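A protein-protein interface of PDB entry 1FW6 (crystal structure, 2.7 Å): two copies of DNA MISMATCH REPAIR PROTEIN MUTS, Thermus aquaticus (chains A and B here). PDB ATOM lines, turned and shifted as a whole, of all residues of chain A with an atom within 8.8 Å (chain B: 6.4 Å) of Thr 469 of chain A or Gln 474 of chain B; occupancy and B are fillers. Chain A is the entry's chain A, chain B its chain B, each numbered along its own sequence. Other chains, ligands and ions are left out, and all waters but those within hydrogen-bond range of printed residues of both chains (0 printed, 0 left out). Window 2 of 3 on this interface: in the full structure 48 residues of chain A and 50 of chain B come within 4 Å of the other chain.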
ATOM      1  N   PHE A 446     -12.194  18.935  -5.331  1.00  0.00           N
ATOM      2  CA  PHE A 446     -11.516  17.850  -4.630  1.00  0.00           C
ATOM      3  C   PHE A 446     -10.060  18.100  -4.273  1.00  0.00           C
ATOM      4  O   PHE A 446      -9.437  17.274  -3.597  1.00  0.00           O
ATOM      5  CB  PHE A 446     -11.586  16.554  -5.444  1.00  0.00           C
ATOM      6  CG  PHE A 446     -12.962  16.202  -5.921  1.00  0.00           C
ATOM      7  CD1 PHE A 446     -13.487  16.793  -7.067  1.00  0.00           C
ATOM      8  CD2 PHE A 446     -13.733  15.268  -5.236  1.00  0.00           C
ATOM      9  CE1 PHE A 446     -14.767  16.456  -7.522  1.00  0.00           C
ATOM     10  CE2 PHE A 446     -15.008  14.928  -5.682  1.00  0.00           C
ATOM     11  CZ  PHE A 446     -15.527  15.523  -6.831  1.00  0.00           C
ATOM     12  N   VAL A 452      -6.308   8.445 -13.178  1.00  0.00           N
ATOM     13  CA  VAL A 452      -6.032   7.232 -13.940  1.00  0.00           C
ATOM     14  C   VAL A 452      -7.222   6.776 -14.781  1.00  0.00           C
ATOM     15  O   VAL A 452      -8.361   6.732 -14.304  1.00  0.00           O
ATOM     16  CB  VAL A 452      -5.587   6.087 -13.001  1.00  0.00           C
ATOM     17  CG1 VAL A 452      -5.811   4.729 -13.658  1.00  0.00           C
ATOM     18  CG2 VAL A 452      -4.113   6.256 -12.672  1.00  0.00           C
ATOM     19  N   ARG A 454      -9.525   4.198 -17.463  1.00  0.00           N
ATOM     20  CA  ARG A 454     -10.189   2.905 -17.349  1.00  0.00           C
ATOM     21  C   ARG A 454      -9.287   1.705 -17.637  1.00  0.00           C
ATOM     22  O   ARG A 454      -9.270   0.736 -16.876  1.00  0.00           O
ATOM     23  CB  ARG A 454     -11.408   2.886 -18.278  1.00  0.00           C
ATOM     24  CG  ARG A 454     -12.170   1.577 -18.301  1.00  0.00           C
ATOM     25  CD  ARG A 454     -13.439   1.699 -19.115  1.00  0.00           C
ATOM     26  NE  ARG A 454     -14.405   2.622 -18.520  1.00  0.00           N
ATOM     27  CZ  ARG A 454     -15.130   2.371 -17.428  1.00  0.00           C
ATOM     28  NH1 ARG A 454     -15.006   1.216 -16.790  1.00  0.00           N
ATOM     29  NH2 ARG A 454     -15.979   3.283 -16.968  1.00  0.00           N
ATOM     30  N   TYR A 457      -7.590   0.580 -14.534  1.00  0.00           N
ATOM     31  CA  TYR A 457      -8.280   0.492 -13.248  1.00  0.00           C
ATOM     32  C   TYR A 457      -7.805  -0.711 -12.419  1.00  0.00           C
ATOM     33  O   TYR A 457      -7.573  -0.591 -11.219  1.00  0.00           O
ATOM     34  CB  TYR A 457      -9.804   0.412 -13.441  1.00  0.00           C
ATOM     35  CG  TYR A 457     -10.486   1.707 -13.834  1.00  0.00           C
ATOM     36  CD1 TYR A 457      -9.783   2.911 -13.908  1.00  0.00           C
ATOM     37  CD2 TYR A 457     -11.844   1.726 -14.136  1.00  0.00           C
ATOM     38  CE1 TYR A 457     -10.419   4.092 -14.275  1.00  0.00           C
ATOM     39  CE2 TYR A 457     -12.487   2.896 -14.502  1.00  0.00           C
ATOM     40  CZ  TYR A 457     -11.772   4.076 -14.569  1.00  0.00           C
ATOM     41  OH  TYR A 457     -12.425   5.236 -14.918  1.00  0.00           O
ATOM     42  N   PRO A 466     -10.050   6.448  -3.503  1.00  0.00           N
ATOM     43  CA  PRO A 466     -11.001   7.008  -4.475  1.00  0.00           C
ATOM     44  C   PRO A 466     -11.524   8.345  -3.969  1.00  0.00           C
ATOM     45  O   PRO A 466     -11.837   8.491  -2.787  1.00  0.00           O
ATOM     46  CB  PRO A 466     -12.110   5.959  -4.532  1.00  0.00           C
ATOM     47  CG  PRO A 466     -11.401   4.691  -4.183  1.00  0.00           C
ATOM     48  CD  PRO A 466     -10.486   5.116  -3.055  1.00  0.00           C
ATOM     49  N   VAL A 467     -11.621   9.317  -4.864  1.00  0.00           N
ATOM     50  CA  VAL A 467     -12.094  10.636  -4.488  1.00  0.00           C
ATOM     51  C   VAL A 467     -13.172  11.099  -5.457  1.00  0.00           C
ATOM     52  O   VAL A 467     -14.167  11.704  -5.049  1.00  0.00           O
ATOM     53  CB  VAL A 467     -10.928  11.644  -4.477  1.00  0.00           C
ATOM     54  CG1 VAL A 467     -11.416  13.006  -4.036  1.00  0.00           C
ATOM     55  CG2 VAL A 467      -9.839  11.157  -3.537  1.00  0.00           C
ATOM     56  N   GLN A 468     -12.975  10.805  -6.741  1.00  0.00           N
ATOM     57  CA  GLN A 468     -13.943  11.192  -7.760  1.00  0.00           C
ATOM     58  C   GLN A 468     -13.958  10.228  -8.948  1.00  0.00           C
ATOM     59  O   GLN A 468     -12.902   9.763  -9.395  1.00  0.00           O
ATOM     60  CB  GLN A 468     -13.651  12.613  -8.255  1.00  0.00           C
ATOM     61  CG  GLN A 468     -14.653  13.097  -9.300  1.00  0.00           C
ATOM     62  CD  GLN A 468     -14.266  14.409  -9.951  1.00  0.00           C
ATOM     63  OE1 GLN A 468     -14.981  14.909 -10.820  1.00  0.00           O
ATOM     64  NE2 GLN A 468     -13.131  14.971  -9.538  1.00  0.00           N
ATOM     65  N   THR A 469     -15.162   9.940  -9.448  1.00  0.00           N
ATOM     66  CA  THR A 469     -15.359   9.039 -10.587  1.00  0.00           C
ATOM     67  C   THR A 469     -15.919   9.794 -11.792  1.00  0.00           C
ATOM     68  O   THR A 469     -16.804  10.639 -11.658  1.00  0.00           O
ATOM     69  CB  THR A 469     -16.359   7.902 -10.264  1.00  0.00           C
ATOM     70  OG1 THR A 469     -15.941   7.203  -9.087  1.00  0.00           O
ATOM     71  CG2 THR A 469     -16.440   6.927 -11.420  1.00  0.00           C
ATOM     72  N   LEU A 470     -15.406   9.481 -12.970  1.00  0.00           N
ATOM     73  CA  LEU A 470     -15.878  10.131 -14.176  1.00  0.00           C
ATOM     74  C   LEU A 470     -16.203   9.075 -15.218  1.00  0.00           C
ATOM     75  O   LEU A 470     -15.992   7.890 -14.976  1.00  0.00           O
ATOM     76  CB  LEU A 470     -14.825  11.108 -14.688  1.00  0.00           C
ATOM     77  CG  LEU A 470     -14.544  12.267 -13.728  1.00  0.00           C
ATOM     78  CD1 LEU A 470     -13.459  11.884 -12.749  1.00  0.00           C
ATOM     79  CD2 LEU A 470     -14.121  13.482 -14.519  1.00  0.00           C
ATOM     80  N   LYS A 471     -16.718   9.494 -16.370  1.00  0.00           N
ATOM     81  CA  LYS A 471     -17.087   8.552 -17.425  1.00  0.00           C
ATOM     82  C   LYS A 471     -16.030   7.464 -17.645  1.00  0.00           C
ATOM     83  O   LYS A 471     -16.351   6.276 -17.673  1.00  0.00           O
ATOM     84  CB  LYS A 471     -17.353   9.295 -18.736  1.00  0.00           C
ATOM     85  CG  LYS A 471     -18.144   8.493 -19.765  1.00  0.00           C
ATOM     86  CD  LYS A 471     -19.543   8.175 -19.251  1.00  0.00           C
ATOM     87  CE  LYS A 471     -20.493   7.723 -20.370  1.00  0.00           C
ATOM     88  NZ  LYS A 471     -20.118   6.450 -21.044  1.00  0.00           N
ATOM     89  N   ASP A 472     -14.774   7.856 -17.798  1.00  0.00           N
ATOM     90  CA  ASP A 472     -13.725   6.867 -17.999  1.00  0.00           C
ATOM     91  C   ASP A 472     -12.398   7.318 -17.426  1.00  0.00           C
ATOM     92  O   ASP A 472     -11.348   7.209 -18.054  1.00  0.00           O
ATOM     93  CB  ASP A 472     -13.597   6.526 -19.480  1.00  0.00           C
ATOM     94  CG  ASP A 472     -14.873   5.923 -20.042  1.00  0.00           C
ATOM     95  OD1 ASP A 472     -15.267   4.822 -19.595  1.00  0.00           O
ATOM     96  OD2 ASP A 472     -15.485   6.563 -20.924  1.00  0.00           O
ATOM     97  N   ARG A 473     -12.488   7.839 -16.211  1.00  0.00           N
ATOM     98  CA  ARG A 473     -11.352   8.299 -15.444  1.00  0.00           C
ATOM     99  C   ARG A 473     -11.765   8.216 -13.985  1.00  0.00           C
ATOM    100  O   ARG A 473     -12.932   8.425 -13.645  1.00  0.00           O
ATOM    101  CB  ARG A 473     -10.994   9.738 -15.793  1.00  0.00           C
ATOM    102  CG  ARG A 473     -10.232   9.895 -17.083  1.00  0.00           C
ATOM    103  CD  ARG A 473     -10.017  11.360 -17.378  1.00  0.00           C
ATOM    104  NE  ARG A 473     -11.279  12.098 -17.436  1.00  0.00           N
ATOM    105  CZ  ARG A 473     -11.381  13.404 -17.659  1.00  0.00           C
ATOM    106  NH1 ARG A 473     -10.295  14.132 -17.852  1.00  0.00           N
ATOM    107  NH2 ARG A 473     -12.571  13.979 -17.683  1.00  0.00           N
ATOM    108  N   GLN A 474     -10.792   7.896 -13.137  1.00  0.00           N
ATOM    109  CA  GLN A 474     -10.993   7.771 -11.699  1.00  0.00           C
ATOM    110  C   GLN A 474      -9.895   8.584 -11.030  1.00  0.00           C
ATOM    111  O   GLN A 474      -8.772   8.626 -11.524  1.00  0.00           O
ATOM    112  CB  GLN A 474     -10.871   6.305 -11.292  1.00  0.00           C
ATOM    113  CG  GLN A 474     -11.201   6.031  -9.846  1.00  0.00           C
ATOM    114  CD  GLN A 474     -12.672   6.208  -9.541  1.00  0.00           C
ATOM    115  OE1 GLN A 474     -13.530   5.559 -10.158  1.00  0.00           O
ATOM    116  NE2 GLN A 474     -12.979   7.087  -8.579  1.00  0.00           N
ATOM    117  N   ARG A 475     -10.212   9.233  -9.914  1.00  0.00           N
ATOM    118  CA  ARG A 475      -9.222  10.048  -9.209  1.00  0.00           C
ATOM    119  C   ARG A 475      -9.015   9.614  -7.763  1.00  0.00           C
ATOM    120  O   ARG A 475      -9.969   9.478  -7.002  1.00  0.00           O
ATOM    121  CB  ARG A 475      -9.628  11.518  -9.284  1.00  0.00           C
ATOM    122  CG  ARG A 475      -9.668  12.041 -10.719  1.00  0.00           C
ATOM    123  CD  ARG A 475     -10.147  13.482 -10.806  1.00  0.00           C
ATOM    124  NE  ARG A 475     -10.182  13.931 -12.192  1.00  0.00           N
ATOM    125  CZ  ARG A 475     -10.869  14.984 -12.610  1.00  0.00           C
ATOM    126  NH1 ARG A 475     -11.564  15.695 -11.746  1.00  0.00           N
ATOM    127  NH2 ARG A 475     -10.890  15.300 -13.894  1.00  0.00           N
ATOM    128  N   TYR A 476      -7.748   9.406  -7.405  1.00  0.00           N
ATOM    129  CA  TYR A 476      -7.359   8.947  -6.074  1.00  0.00           C
ATOM    130  C   TYR A 476      -6.558   9.945  -5.271  1.00  0.00           C
ATOM    131  O   TYR A 476      -6.252  11.038  -5.731  1.00  0.00           O
ATOM    132  CB  TYR A 476      -6.540   7.663  -6.181  1.00  0.00           C
ATOM    133  CG  TYR A 476      -7.145   6.675  -7.134  1.00  0.00           C
ATOM    134  CD1 TYR A 476      -6.900   6.770  -8.508  1.00  0.00           C
ATOM    135  CD2 TYR A 476      -8.023   5.688  -6.681  1.00  0.00           C
ATOM    136  CE1 TYR A 476      -7.514   5.910  -9.406  1.00  0.00           C
ATOM    137  CE2 TYR A 476      -8.644   4.826  -7.573  1.00  0.00           C
ATOM    138  CZ  TYR A 476      -8.386   4.945  -8.934  1.00  0.00           C
ATOM    139  OH  TYR A 476      -9.013   4.109  -9.824  1.00  0.00           O
ATOM    140  N   LEU B 450     -28.704   7.625  -9.132  1.00  0.00           N
ATOM    141  CA  LEU B 450     -28.980   7.596  -7.702  1.00  0.00           C
ATOM    142  C   LEU B 450     -28.001   8.581  -7.084  1.00  0.00           C
ATOM    143  O   LEU B 450     -26.840   8.629  -7.478  1.00  0.00           O
ATOM    144  CB  LEU B 450     -28.744   6.194  -7.138  1.00  0.00           C
ATOM    145  CG  LEU B 450     -29.733   5.127  -7.620  1.00  0.00           C
ATOM    146  CD1 LEU B 450     -29.159   3.748  -7.387  1.00  0.00           C
ATOM    147  CD2 LEU B 450     -31.070   5.288  -6.911  1.00  0.00           C
ATOM    148  N   GLU B 451     -28.464   9.374  -6.125  1.00  0.00           N
ATOM    149  CA  GLU B 451     -27.600  10.366  -5.501  1.00  0.00           C
ATOM    150  C   GLU B 451     -27.471  10.168  -3.990  1.00  0.00           C
ATOM    151  O   GLU B 451     -28.457  10.237  -3.255  1.00  0.00           O
ATOM    152  CB  GLU B 451     -28.142  11.760  -5.799  1.00  0.00           C
ATOM    153  CG  GLU B 451     -27.140  12.877  -5.658  1.00  0.00           C
ATOM    154  CD  GLU B 451     -27.797  14.235  -5.769  1.00  0.00           C
ATOM    155  OE1 GLU B 451     -28.437  14.665  -4.785  1.00  0.00           O
ATOM    156  OE2 GLU B 451     -27.690  14.869  -6.840  1.00  0.00           O
ATOM    157  N   VAL B 452     -26.246   9.930  -3.534  1.00  0.00           N
ATOM    158  CA  VAL B 452     -25.980   9.713  -2.118  1.00  0.00           C
ATOM    159  C   VAL B 452     -25.071  10.797  -1.550  1.00  0.00           C
ATOM    160  O   VAL B 452     -24.080  11.162  -2.171  1.00  0.00           O
ATOM    161  CB  VAL B 452     -25.310   8.342  -1.888  1.00  0.00           C
ATOM    162  CG1 VAL B 452     -24.923   8.192  -0.428  1.00  0.00           C
ATOM    163  CG2 VAL B 452     -26.252   7.223  -2.296  1.00  0.00           C
ATOM    164  N   THR B 453     -25.405  11.305  -0.367  1.00  0.00           N
ATOM    165  CA  THR B 453     -24.595  12.342   0.267  1.00  0.00           C
ATOM    166  C   THR B 453     -23.316  11.742   0.852  1.00  0.00           C
ATOM    167  O   THR B 453     -23.209  10.528   1.019  1.00  0.00           O
ATOM    168  CB  THR B 453     -25.366  13.062   1.398  1.00  0.00           C
ATOM    169  OG1 THR B 453     -25.551  12.169   2.501  1.00  0.00           O
ATOM    170  CG2 THR B 453     -26.728  13.530   0.900  1.00  0.00           C
ATOM    171  N   ARG B 454     -22.353  12.602   1.164  1.00  0.00           N
ATOM    172  CA  ARG B 454     -21.062  12.185   1.714  1.00  0.00           C
ATOM    173  C   ARG B 454     -21.159  11.240   2.923  1.00  0.00           C
ATOM    174  O   ARG B 454     -20.499  10.201   2.964  1.00  0.00           O
ATOM    175  CB  ARG B 454     -20.247  13.431   2.107  1.00  0.00           C
ATOM    176  CG  ARG B 454     -18.729  13.318   1.946  1.00  0.00           C
ATOM    177  CD  ARG B 454     -18.148  12.125   2.690  1.00  0.00           C
ATOM    178  NE  ARG B 454     -16.694  12.013   2.554  1.00  0.00           N
ATOM    179  CZ  ARG B 454     -16.025  12.068   1.400  1.00  0.00           C
ATOM    180  NH1 ARG B 454     -16.669  12.243   0.252  1.00  0.00           N
ATOM    181  NH2 ARG B 454     -14.704  11.932   1.393  1.00  0.00           N
ATOM    182  N   TYR B 457     -21.678   7.047   2.561  1.00  0.00           N
ATOM    183  CA  TYR B 457     -20.848   6.209   1.698  1.00  0.00           C
ATOM    184  C   TYR B 457     -20.621   4.823   2.301  1.00  0.00           C
ATOM    185  O   TYR B 457     -20.394   3.848   1.574  1.00  0.00           O
ATOM    186  CB  TYR B 457     -19.496   6.876   1.416  1.00  0.00           C
ATOM    187  CG  TYR B 457     -19.579   8.105   0.538  1.00  0.00           C
ATOM    188  CD1 TYR B 457     -20.370   8.118  -0.610  1.00  0.00           C
ATOM    189  CD2 TYR B 457     -18.847   9.248   0.842  1.00  0.00           C
ATOM    190  CE1 TYR B 457     -20.427   9.246  -1.435  1.00  0.00           C
ATOM    191  CE2 TYR B 457     -18.898  10.378   0.025  1.00  0.00           C
ATOM    192  CZ  TYR B 457     -19.688  10.373  -1.110  1.00  0.00           C
ATOM    193  OH  TYR B 457     -19.720  11.489  -1.919  1.00  0.00           O
ATOM    194  N   PRO B 466     -20.777   3.781  -9.142  1.00  0.00           N
ATOM    195  CA  PRO B 466     -20.604   5.233  -9.251  1.00  0.00           C
ATOM    196  C   PRO B 466     -20.372   5.679 -10.691  1.00  0.00           C
ATOM    197  O   PRO B 466     -19.774   4.953 -11.490  1.00  0.00           O
ATOM    198  CB  PRO B 466     -19.411   5.514  -8.331  1.00  0.00           C
ATOM    199  CG  PRO B 466     -18.649   4.221  -8.346  1.00  0.00           C
ATOM    200  CD  PRO B 466     -19.755   3.199  -8.256  1.00  0.00           C
ATOM    201  N   VAL B 467     -20.861   6.873 -11.011  1.00  0.00           N
ATOM    202  CA  VAL B 467     -20.740   7.427 -12.357  1.00  0.00           C
ATOM    203  C   VAL B 467     -20.242   8.856 -12.299  1.00  0.00           C
ATOM    204  O   VAL B 467     -19.718   9.382 -13.284  1.00  0.00           O
ATOM    205  CB  VAL B 467     -22.108   7.474 -13.080  1.00  0.00           C
ATOM    206  CG1 VAL B 467     -21.911   7.816 -14.541  1.00  0.00           C
ATOM    207  CG2 VAL B 467     -22.832   6.161 -12.923  1.00  0.00           C
ATOM    208  N   GLN B 468     -20.411   9.478 -11.139  1.00  0.00           N
ATOM    209  CA  GLN B 468     -20.026  10.867 -10.974  1.00  0.00           C
ATOM    210  C   GLN B 468     -20.032  11.278  -9.498  1.00  0.00           C
ATOM    211  O   GLN B 468     -21.006  11.030  -8.781  1.00  0.00           O
ATOM    212  CB  GLN B 468     -21.009  11.719 -11.780  1.00  0.00           C
ATOM    213  CG  GLN B 468     -20.897  13.212 -11.613  1.00  0.00           C
ATOM    214  CD  GLN B 468     -22.028  13.928 -12.318  1.00  0.00           C
ATOM    215  OE1 GLN B 468     -23.205  13.698 -12.020  1.00  0.00           O
ATOM    216  NE2 GLN B 468     -21.683  14.795 -13.264  1.00  0.00           N
ATOM    217  N   THR B 469     -18.944  11.904  -9.049  1.00  0.00           N
ATOM    218  CA  THR B 469     -18.826  12.346  -7.661  1.00  0.00           C
ATOM    219  C   THR B 469     -18.844  13.873  -7.561  1.00  0.00           C
ATOM    220  O   THR B 469     -18.205  14.569  -8.354  1.00  0.00           O
ATOM    221  CB  THR B 469     -17.517  11.831  -7.014  1.00  0.00           C
ATOM    222  OG1 THR B 469     -17.327  10.449  -7.336  1.00  0.00           O
ATOM    223  CG2 THR B 469     -17.583  11.974  -5.503  1.00  0.00           C
ATOM    224  N   LEU B 470     -19.580  14.387  -6.581  1.00  0.00           N
ATOM    225  CA  LEU B 470     -19.683  15.825  -6.370  1.00  0.00           C
ATOM    226  C   LEU B 470     -19.102  16.230  -5.019  1.00  0.00           C
ATOM    227  O   LEU B 470     -18.700  15.380  -4.225  1.00  0.00           O
ATOM    228  CB  LEU B 470     -21.146  16.277  -6.463  1.00  0.00           C
ATOM    229  CG  LEU B 470     -21.813  16.233  -7.842  1.00  0.00           C
ATOM    230  CD1 LEU B 470     -21.825  14.810  -8.371  1.00  0.00           C
ATOM    231  CD2 LEU B 470     -23.230  16.775  -7.744  1.00  0.00           C
ATOM    232  N   ASP B 472     -20.365  17.405  -2.092  1.00  0.00           N
ATOM    233  CA  ASP B 472     -20.951  16.797  -0.907  1.00  0.00           C
ATOM    234  C   ASP B 472     -21.733  15.517  -1.140  1.00  0.00           C
ATOM    235  O   ASP B 472     -22.292  14.963  -0.197  1.00  0.00           O
ATOM    236  CB  ASP B 472     -21.841  17.804  -0.173  1.00  0.00           C
ATOM    237  CG  ASP B 472     -22.747  18.580  -1.108  1.00  0.00           C
ATOM    238  OD1 ASP B 472     -22.242  19.499  -1.792  1.00  0.00           O
ATOM    239  OD2 ASP B 472     -23.958  18.267  -1.158  1.00  0.00           O
ATOM    240  N   ARG B 473     -21.782  15.047  -2.384  1.00  0.00           N
ATOM    241  CA  ARG B 473     -22.497  13.808  -2.694  1.00  0.00           C
ATOM    242  C   ARG B 473     -22.008  13.166  -3.991  1.00  0.00           C
ATOM    243  O   ARG B 473     -21.312  13.792  -4.784  1.00  0.00           O
ATOM    244  CB  ARG B 473     -24.017  14.046  -2.754  1.00  0.00           C
ATOM    245  CG  ARG B 473     -24.513  14.862  -3.929  1.00  0.00           C
ATOM    246  CD  ARG B 473     -24.069  16.311  -3.857  1.00  0.00           C
ATOM    247  NE  ARG B 473     -24.452  17.031  -5.066  1.00  0.00           N
ATOM    248  CZ  ARG B 473     -25.704  17.327  -5.394  1.00  0.00           C
ATOM    249  NH1 ARG B 473     -26.706  16.970  -4.593  1.00  0.00           N
ATOM    250  NH2 ARG B 473     -25.955  17.955  -6.535  1.00  0.00           N
ATOM    251  N   GLN B 474     -22.379  11.908  -4.198  1.00  0.00           N
ATOM    252  CA  GLN B 474     -21.951  11.162  -5.372  1.00  0.00           C
ATOM    253  C   GLN B 474     -23.136  10.420  -5.980  1.00  0.00           C
ATOM    254  O   GLN B 474     -23.939   9.826  -5.260  1.00  0.00           O
ATOM    255  CB  GLN B 474     -20.846  10.181  -4.953  1.00  0.00           C
ATOM    256  CG  GLN B 474     -20.189   9.402  -6.083  1.00  0.00           C
ATOM    257  CD  GLN B 474     -18.935   8.656  -5.636  1.00  0.00           C
ATOM    258  OE1 GLN B 474     -18.369   7.860  -6.393  1.00  0.00           O
ATOM    259  NE2 GLN B 474     -18.492   8.920  -4.407  1.00  0.00           N
ATOM    260  N   ARG B 475     -23.235  10.455  -7.307  1.00  0.00           N
ATOM    261  CA  ARG B 475     -24.331   9.808  -8.029  1.00  0.00           C
ATOM    262  C   ARG B 475     -23.955   8.445  -8.617  1.00  0.00           C
ATOM    263  O   ARG B 475     -22.996   8.339  -9.386  1.00  0.00           O
ATOM    264  CB  ARG B 475     -24.812  10.735  -9.146  1.00  0.00           C
ATOM    265  CG  ARG B 475     -25.225  12.112  -8.648  1.00  0.00           C
ATOM    266  CD  ARG B 475     -25.382  13.115  -9.782  1.00  0.00           C
ATOM    267  NE  ARG B 475     -25.699  14.447  -9.272  1.00  0.00           N
ATOM    268  CZ  ARG B 475     -25.824  15.533 -10.027  1.00  0.00           C
ATOM    269  NH1 ARG B 475     -25.661  15.448 -11.340  1.00  0.00           N
ATOM    270  NH2 ARG B 475     -26.107  16.704  -9.468  1.00  0.00           N
ATOM    271  N   TYR B 476     -24.722   7.411  -8.258  1.00  0.00           N
ATOM    272  CA  TYR B 476     -24.479   6.045  -8.736  1.00  0.00           C
ATOM    273  C   TYR B 476     -25.488   5.585  -9.799  1.00  0.00           C
ATOM    274  O   TYR B 476     -26.440   6.296 -10.125  1.00  0.00           O
ATOM    275  CB  TYR B 476     -24.534   5.033  -7.583  1.00  0.00           C
ATOM    276  CG  TYR B 476     -23.630   5.295  -6.399  1.00  0.00           C
ATOM    277  CD1 TYR B 476     -23.889   6.340  -5.509  1.00  0.00           C
ATOM    278  CD2 TYR B 476     -22.560   4.446  -6.120  1.00  0.00           C
ATOM    279  CE1 TYR B 476     -23.110   6.525  -4.362  1.00  0.00           C
ATOM    280  CE2 TYR B 476     -21.776   4.623  -4.979  1.00  0.00           C
ATOM    281  CZ  TYR B 476     -22.060   5.659  -4.103  1.00  0.00           C
ATOM    282  OH  TYR B 476     -21.318   5.798  -2.955  1.00  0.00           O
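N of Val 467 of chain A sits at hydrogen-bond distance from O of Arg 475 of chain A (2.7 Å).
NE2 of Gln 474 of chain A is in hydrogen-bond range of O of Gln 468 of chain A (2.8 Å).
The backbone carbonyl oxygen of Gln 468 of chain A lies within hydrogen-bond range of the backbone NH of Arg 475 of chain A (2.8 Å).
The backbone carbonyl oxygen (O) of Val 452 of chain B sits at hydrogen-bond distance from the backbone NH (N) of Gln 474 of chain B, 2.7 Å away.
O of Gln 468 of chain B sits at hydrogen-bond distance from N of Arg 475 of chain B, at 2.7 Å.
The side-chain hydroxyl (OG1) of Thr 469 of chain B is in hydrogen-bond range of the side-chain amide oxygen (OE1) of Gln 474 of chain B (2.9 Å).
The backbone NH of Thr 469 of chain A lies within hydrogen-bond range of the side-chain hydroxyl of Thr 469 of chain B (3.1 Å).
Phe 446 of chain A touches Thr 469 of chain B.
Leu 470 of chain B touches Phe 446 of chain A.
Val 467 of chain A touches Thr 469 of chain B (O to CG2, 3.5 Å).
Gln 468 of chain A touches Thr 469 of chain B (CA to OG1, 3.5 Å).
Thr 469 of chain A touches Pro 466 of chain B (CG2 to O, 3.9 Å).
O of Val 467 of chain B touches O of Thr 469 of chain A, at 3.6 Å.
CA of Gln 468 of chain B touches O of Thr 469 of chain A (3.3 Å).
OG1 of Thr 469 of chain A touches OE1 of Gln 474 of chain B, 3.7 Å away.
Val 467 of chain A touches Thr 469 of chain B, and with the chains exchanged Thr 469 of chain A touches Val 467 of chain B.
Gln 468 of chain A touches Thr 469 of chain B, and with the chains exchanged Thr 469 of chain A touches Gln 468 of chain B.
Thr 469 of chain A touches Pro 466 of chain B, but with the chains exchanged Pro 466 of chain A does not touch Thr 469 of chain B (7.0 Å).
Thr 469 of chain A touches Gln 474 of chain B, but with the chains exchanged Gln 474 of chain A does not touch Thr 469 of chain B (5.6 Å).
Thr 469 of chain A touches just these residues of chain B: Pro 466, Val 467, Gln 468, Thr 469 and Gln 474.
Gln 474 of chain B touches just one residue of chain A: Thr 469 (3.7 Å).
Printed residues of chain A within 4 Å of Pro 466 of chain B: Thr 469 (3.9 Å).
Printed residues of chain A within 4 Å of Thr 469 of chain B: Phe 446 (3.2 Å), Val 467 (3.5 Å), Gln 468 (3.5 Å) and Thr 469 (3.1 Å).
Printed residues of chain A within 4 Å of Val 467 of chain B: Thr 469.
Printed residues of chain B within 4 Å of Gln 468 of chain A: Thr 469 (3.5 Å).
Gln 474 of chain A touches none of the printed residues of chain B.
Arg 475 of chain A touches none of the printed residues of chain B.
The nearest printed residue of chain B that does not touch Thr 469 of chain A is Arg 475 of chain B (6.7 Å).
The nearest residue of chain A that does not touch Gln 474 of chain B is Val 467 of chain A (5.2 Å).
Of the 16 printed residues of chain B, 6 touch a printed residue of chain A.
Hydrophobic or aromatic side chains of chain A that line the printed part of chain B: Phe 446.
Among the printed residues, 9 pairs touch across the chains.
Among the printed residues, no Asp or Glu carboxylate lies within 4 Å of a Lys or Arg side-chain nitrogen of the other chain.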
